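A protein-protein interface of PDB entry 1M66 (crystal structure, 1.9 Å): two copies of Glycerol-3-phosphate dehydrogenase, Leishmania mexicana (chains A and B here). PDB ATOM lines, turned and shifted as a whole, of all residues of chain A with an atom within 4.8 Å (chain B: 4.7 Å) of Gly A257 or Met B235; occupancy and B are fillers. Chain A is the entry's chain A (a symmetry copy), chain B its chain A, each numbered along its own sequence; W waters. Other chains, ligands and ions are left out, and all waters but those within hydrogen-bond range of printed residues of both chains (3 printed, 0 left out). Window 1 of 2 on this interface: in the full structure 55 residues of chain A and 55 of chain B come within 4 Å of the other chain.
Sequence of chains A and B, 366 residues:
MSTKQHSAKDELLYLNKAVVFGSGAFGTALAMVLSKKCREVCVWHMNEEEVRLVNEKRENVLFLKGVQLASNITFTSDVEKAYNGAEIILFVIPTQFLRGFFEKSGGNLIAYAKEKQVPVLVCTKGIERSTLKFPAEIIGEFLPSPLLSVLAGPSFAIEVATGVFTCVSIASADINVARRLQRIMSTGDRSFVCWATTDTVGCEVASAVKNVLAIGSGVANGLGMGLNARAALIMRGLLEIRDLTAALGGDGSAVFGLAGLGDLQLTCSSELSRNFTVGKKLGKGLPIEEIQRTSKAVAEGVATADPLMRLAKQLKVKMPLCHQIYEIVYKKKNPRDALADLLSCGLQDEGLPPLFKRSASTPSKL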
ATOM      1  N   SER A 253     -30.741  14.413  30.644  1.00  0.00           N
ATOM      2  CA  SER A 253     -30.300  14.006  29.305  1.00  0.00           C
ATOM      3  C   SER A 253     -28.777  14.147  29.054  1.00  0.00           C
ATOM      4  O   SER A 253     -28.247  13.531  28.118  1.00  0.00           O
ATOM      5  CB  SER A 253     -31.122  14.706  28.211  1.00  0.00           C
ATOM      6  OG  SER A 253     -30.909  16.108  28.239  1.00  0.00           O
ATOM      7  N   ALA A 254     -28.072  14.904  29.888  1.00  0.00           N
ATOM      8  CA  ALA A 254     -26.618  15.049  29.732  1.00  0.00           C
ATOM      9  C   ALA A 254     -25.833  13.978  30.458  1.00  0.00           C
ATOM     10  O   ALA A 254     -24.649  13.758  30.174  1.00  0.00           O
ATOM     11  CB  ALA A 254     -26.144  16.408  30.203  1.00  0.00           C
ATOM     12  N   VAL A 255     -26.492  13.299  31.386  1.00  0.00           N
ATOM     13  CA  VAL A 255     -25.808  12.297  32.203  1.00  0.00           C
ATOM     14  C   VAL A 255     -25.014  11.258  31.417  1.00  0.00           C
ATOM     15  O   VAL A 255     -23.876  10.950  31.757  1.00  0.00           O
ATOM     16  CB  VAL A 255     -26.798  11.600  33.151  1.00  0.00           C
ATOM     17  CG1 VAL A 255     -26.144  10.415  33.861  1.00  0.00           C
ATOM     18  CG2 VAL A 255     -27.359  12.618  34.148  1.00  0.00           C
ATOM     19  N   PHE A 256     -25.635  10.675  30.397  1.00  0.00           N
ATOM     20  CA  PHE A 256     -24.962   9.666  29.588  1.00  0.00           C
ATOM     21  C   PHE A 256     -24.339  10.244  28.338  1.00  0.00           C
ATOM     22  O   PHE A 256     -24.089   9.526  27.374  1.00  0.00           O
ATOM     23  CB  PHE A 256     -25.945   8.558  29.216  1.00  0.00           C
ATOM     24  CG  PHE A 256     -26.404   7.788  30.409  1.00  0.00           C
ATOM     25  CD1 PHE A 256     -27.693   7.884  30.846  1.00  0.00           C
ATOM     26  CD2 PHE A 256     -25.497   7.040  31.151  1.00  0.00           C
ATOM     27  CE1 PHE A 256     -28.120   7.202  31.966  1.00  0.00           C
ATOM     28  CE2 PHE A 256     -25.918   6.354  32.279  1.00  0.00           C
ATOM     29  CZ  PHE A 256     -27.220   6.442  32.687  1.00  0.00           C
ATOM     30  N   GLY A 257     -24.111  11.540  28.342  1.00  0.00           N
ATOM     31  CA  GLY A 257     -23.475  12.151  27.190  1.00  0.00           C
ATOM     32  C   GLY A 257     -22.091  12.673  27.508  1.00  0.00           C
ATOM     33  O   GLY A 257     -21.440  12.260  28.483  1.00  0.00           O
ATOM     34  N   LEU A 258     -21.632  13.600  26.669  1.00  0.00           N
ATOM     35  CA  LEU A 258     -20.288  14.155  26.817  1.00  0.00           C
ATOM     36  C   LEU A 258     -20.034  14.814  28.163  1.00  0.00           C
ATOM     37  O   LEU A 258     -18.960  14.661  28.748  1.00  0.00           O
ATOM     38  CB  LEU A 258     -20.048  15.180  25.685  1.00  0.00           C
ATOM     39  CG  LEU A 258     -19.943  14.629  24.271  1.00  0.00           C
ATOM     40  CD1 LEU A 258     -20.120  15.813  23.260  1.00  0.00           C
ATOM     41  CD2 LEU A 258     -18.585  13.916  24.041  1.00  0.00           C
ATOM     42  N   ALA A 259     -21.003  15.578  28.651  1.00  0.00           N
ATOM     43  CA  ALA A 259     -20.818  16.270  29.911  1.00  0.00           C
ATOM     44  C   ALA A 259     -20.809  15.313  31.090  1.00  0.00           C
ATOM     45  O   ALA A 259     -20.191  15.576  32.111  1.00  0.00           O
ATOM     46  CB  ALA A 259     -21.907  17.339  30.106  1.00  0.00           C
ATOM     47  N   GLY A 260     -21.492  14.188  30.965  1.00  0.00           N
ATOM     48  CA  GLY A 260     -21.558  13.300  32.101  1.00  0.00           C
ATOM     49  C   GLY A 260     -20.518  12.213  31.974  1.00  0.00           C
ATOM     50  O   GLY A 260     -19.368  12.374  32.352  1.00  0.00           O
ATOM     51  N   LEU A 261     -20.941  11.098  31.413  1.00  0.00           N
ATOM     52  CA  LEU A 261     -20.069   9.947  31.244  1.00  0.00           C
ATOM     53  C   LEU A 261     -18.736  10.274  30.535  1.00  0.00           C
ATOM     54  O   LEU A 261     -17.656   9.824  30.954  1.00  0.00           O
ATOM     55  CB  LEU A 261     -20.865   8.897  30.476  1.00  0.00           C
ATOM     56  CG  LEU A 261     -20.226   7.770  29.675  1.00  0.00           C
ATOM     57  CD1 LEU A 261     -18.965   7.143  30.333  1.00  0.00           C
ATOM     58  CD2 LEU A 261     -21.360   6.751  29.395  1.00  0.00           C
ATOM     59  N   GLY A 262     -18.823  11.066  29.481  1.00  0.00           N
ATOM     60  CA  GLY A 262     -17.660  11.417  28.680  1.00  0.00           C
ATOM     61  C   GLY A 262     -16.597  12.096  29.524  1.00  0.00           C
ATOM     62  O   GLY A 262     -15.455  11.633  29.587  1.00  0.00           O
ATOM     63  N   ALA B 231     -12.448   9.989  24.356  1.00  0.00           N
ATOM     64  CA  ALA B 231     -13.672  10.112  25.154  1.00  0.00           C
ATOM     65  C   ALA B 231     -14.909  10.344  24.270  1.00  0.00           C
ATOM     66  O   ALA B 231     -15.960   9.739  24.503  1.00  0.00           O
ATOM     67  CB  ALA B 231     -13.522  11.222  26.153  1.00  0.00           C
ATOM     68  N   ALA B 232     -14.781  11.196  23.250  1.00  0.00           N
ATOM     69  CA  ALA B 232     -15.871  11.464  22.314  1.00  0.00           C
ATOM     70  C   ALA B 232     -16.265  10.229  21.514  1.00  0.00           C
ATOM     71  O   ALA B 232     -17.447   9.984  21.272  1.00  0.00           O
ATOM     72  CB  ALA B 232     -15.510  12.637  21.354  1.00  0.00           C
ATOM     73  N   LEU B 233     -15.267   9.450  21.103  1.00  0.00           N
ATOM     74  CA  LEU B 233     -15.508   8.224  20.348  1.00  0.00           C
ATOM     75  C   LEU B 233     -16.282   7.235  21.202  1.00  0.00           C
ATOM     76  O   LEU B 233     -17.198   6.600  20.708  1.00  0.00           O
ATOM     77  CB  LEU B 233     -14.197   7.592  19.898  1.00  0.00           C
ATOM     78  CG  LEU B 233     -14.344   6.224  19.214  1.00  0.00           C
ATOM     79  CD1 LEU B 233     -13.486   6.152  17.970  1.00  0.00           C
ATOM     80  CD2 LEU B 233     -14.007   5.082  20.181  1.00  0.00           C
ATOM     81  N   ILE B 234     -15.882   7.105  22.464  1.00  0.00           N
ATOM     82  CA  ILE B 234     -16.574   6.230  23.410  1.00  0.00           C
ATOM     83  C   ILE B 234     -18.029   6.657  23.552  1.00  0.00           C
ATOM     84  O   ILE B 234     -18.947   5.834  23.454  1.00  0.00           O
ATOM     85  CB  ILE B 234     -15.878   6.274  24.795  1.00  0.00           C
ATOM     86  CG1 ILE B 234     -14.564   5.486  24.757  1.00  0.00           C
ATOM     87  CG2 ILE B 234     -16.754   5.674  25.864  1.00  0.00           C
ATOM     88  CD1 ILE B 234     -13.675   5.737  25.981  1.00  0.00           C
ATOM     89  N   MET B 235     -18.242   7.950  23.796  1.00  0.00           N
ATOM     90  CA  MET B 235     -19.598   8.440  24.041  1.00  0.00           C
ATOM     91  C   MET B 235     -20.509   8.389  22.830  1.00  0.00           C
ATOM     92  O   MET B 235     -21.676   8.000  22.970  1.00  0.00           O
ATOM     93  CB  MET B 235     -19.598   9.833  24.656  1.00  0.00           C
ATOM     94  CG  MET B 235     -18.795   9.890  25.917  1.00  0.00           C
ATOM     95  SD  MET B 235     -19.219   8.511  27.025  1.00  0.00           S
ATOM     96  CE  MET B 235     -21.076   8.724  27.025  1.00  0.00           C
ATOM     97  N   ARG B 236     -19.994   8.715  21.643  1.00  0.00           N
ATOM     98  CA  ARG B 236     -20.827   8.675  20.443  1.00  0.00           C
ATOM     99  C   ARG B 236     -20.999   7.233  20.007  1.00  0.00           C
ATOM    100  O   ARG B 236     -22.090   6.810  19.568  1.00  0.00           O
ATOM    101  CB  ARG B 236     -20.223   9.507  19.296  1.00  0.00           C
ATOM    102  CG  ARG B 236     -20.038  11.011  19.614  1.00  0.00           C
ATOM    103  CD  ARG B 236     -21.296  11.717  20.060  1.00  0.00           C
ATOM    104  NE  ARG B 236     -22.378  11.536  19.094  1.00  0.00           N
ATOM    105  CZ  ARG B 236     -23.642  11.886  19.308  1.00  0.00           C
ATOM    106  NH1 ARG B 236     -24.003  12.422  20.464  1.00  0.00           N
ATOM    107  NH2 ARG B 236     -24.550  11.711  18.363  1.00  0.00           N
ATOM    108  N   GLY B 237     -19.914   6.468  20.146  1.00  0.00           N
ATOM    109  CA  GLY B 237     -19.937   5.055  19.813  1.00  0.00           C
ATOM    110  C   GLY B 237     -21.003   4.317  20.612  1.00  0.00           C
ATOM    111  O   GLY B 237     -21.686   3.430  20.092  1.00  0.00           O
ATOM    112  N   LEU B 238     -21.165   4.701  21.877  1.00  0.00           N
ATOM    113  CA  LEU B 238     -22.146   4.073  22.766  1.00  0.00           C
ATOM    114  C   LEU B 238     -23.580   4.164  22.227  1.00  0.00           C
ATOM    115  O   LEU B 238     -24.393   3.249  22.423  1.00  0.00           O
ATOM    116  CB  LEU B 238     -22.072   4.693  24.164  1.00  0.00           C
ATOM    117  CG  LEU B 238     -22.870   4.066  25.310  1.00  0.00           C
ATOM    118  CD1 LEU B 238     -22.502   2.603  25.469  1.00  0.00           C
ATOM    119  CD2 LEU B 238     -22.553   4.818  26.587  1.00  0.00           C
ATOM    120  N   LEU B 239     -23.896   5.268  21.557  1.00  0.00           N
ATOM    121  CA  LEU B 239     -25.226   5.416  20.971  1.00  0.00           C
ATOM    122  C   LEU B 239     -25.449   4.411  19.858  1.00  0.00           C
ATOM    123  O   LEU B 239     -26.588   4.048  19.565  1.00  0.00           O
ATOM    124  CB  LEU B 239     -25.441   6.831  20.442  1.00  0.00           C
ATOM    125  CG  LEU B 239     -25.213   7.898  21.514  1.00  0.00           C
ATOM    126  CD1 LEU B 239     -25.719   9.249  21.008  1.00  0.00           C
ATOM    127  CD2 LEU B 239     -25.954   7.501  22.782  1.00  0.00           C
ATOM    128  N   GLU B 350     -27.328  16.526  21.019  1.00  0.00           N
ATOM    129  CA  GLU B 350     -26.630  15.344  21.499  1.00  0.00           C
ATOM    130  C   GLU B 350     -27.342  14.004  21.255  1.00  0.00           C
ATOM    131  O   GLU B 350     -26.694  12.974  21.097  1.00  0.00           O
ATOM    132  CB  GLU B 350     -26.219  15.509  22.969  1.00  0.00           C
ATOM    133  CG  GLU B 350     -25.235  14.451  23.415  1.00  0.00           C
ATOM    134  CD  GLU B 350     -24.409  14.837  24.632  1.00  0.00           C
ATOM    135  OE1 GLU B 350     -24.899  15.558  25.548  1.00  0.00           O
ATOM    136  OE2 GLU B 350     -23.268  14.352  24.692  1.00  0.00           O
ATOM    137  N   LEU B 352     -29.683  12.366  23.217  1.00  0.00           N
ATOM    138  CA  LEU B 352     -30.047  11.594  24.386  1.00  0.00           C
ATOM    139  C   LEU B 352     -31.381  12.106  24.951  1.00  0.00           C
ATOM    140  O   LEU B 352     -31.545  13.307  25.166  1.00  0.00           O
ATOM    141  CB  LEU B 352     -28.960  11.744  25.450  1.00  0.00           C
ATOM    142  CG  LEU B 352     -27.702  10.912  25.231  1.00  0.00           C
ATOM    143  CD1 LEU B 352     -26.559  11.488  26.030  1.00  0.00           C
ATOM    144  CD2 LEU B 352     -27.983   9.458  25.652  1.00  0.00           C
HETATM  145  O   HOH W   1     -23.672  15.741  27.880  1.00  0.00           O
HETATM  146  O   HOH W   2     -23.280   7.610  25.195  1.00  0.00           O
HETATM  147  O   HOH W   3     -27.570  15.560  26.227  1.00  0.00           O
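N of Gly A262 sits at hydrogen-bond distance from SD of Met B235 (3.6 Å).
N of Leu A258 sits at hydrogen-bond distance from OE2 of Glu B350 (2.7 Å).
Printed residues of chain B that touch a printed residue of chain A: Ala B231, Met B235, Leu B238, Glu B350 and Leu B352.
Hydrophobic or aromatic side chains of chain B that line the printed part of chain A: Ala B231, Met B235, Leu B238 and Leu B352.
Hydrophobic or aromatic side chains of chain A within 4 Å of the printed part of chain B: Leu A258 and Leu A261.
Along chain A the printed residues that touch a printed residue of chain B span positions 253 to 262.
Among the printed residues, pairs that only touch across the chains: Leu A261 with Met B235, Phe A256 with Met B235, Ser A253 with Leu B352, Gly A257 with Glu B350, Gly A257 with Leu B352, Phe A256 with Leu B352, Leu A261 with Leu B238, Gly A257 with Met B235 and Gly A262 with Ala B231.
No position is printed for both chains.
Of the 11 pairs that touch across the chains among the printed residues, none has its exchanged pair printed and touching as well.
Of the printed residues of chain B, Ser A253 touches Leu B352 (3.3 Å).
Of chain B, only Met B235 (3.8 Å), Glu B350 (3.3 Å) and Leu B352 (3.4 Å) come within 4 Å of Gly A257.
Met B235 touches just these residues of chain A: Phe A256, Gly A257, Leu A261 and Gly A262.
Of the printed residues of chain A, Leu B238 touches Leu A261.
Of the printed residues of chain A, Glu B350 touches Gly A257 and Leu A258.
The nearest printed residue of chain B that does not touch Gly A257 is Arg B236 (6.8 Å).
The nearest printed residue of chain B that does not touch Leu A258 is Ala B232 (4.04 Å).
Water W1 lies within hydrogen-bond range of the side-chain carboxylate of Glu B350, the backbone NH of Ala A259, the backbone carbonyl oxygen of Ala A254 and the backbone NH of Leu A258.
Water W3 bridges the side-chain carboxylate (OE1) of Glu B350 (2.8 Å) and the backbone carbonyl oxygen (O) of Ser A253 (2.9 Å).
Water W2 lies within hydrogen-bond range of O of Met B235 (2.8 Å) and O of Phe A256 (3.0 Å).
The guanidinium group (NH1) of Arg B236 lies within hydrogen-bond range of the backbone carbonyl oxygen (O) of Glu B350 (2.8 Å).
The backbone carbonyl oxygen of Val A255 is in hydrogen-bond range of the backbone NH of Leu A261 (3.0 Å).
The backbone NH (N) of Gly A262 sits at hydrogen-bond distance from the backbone carbonyl oxygen (O) of Gly A257, 3.0 Å away.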
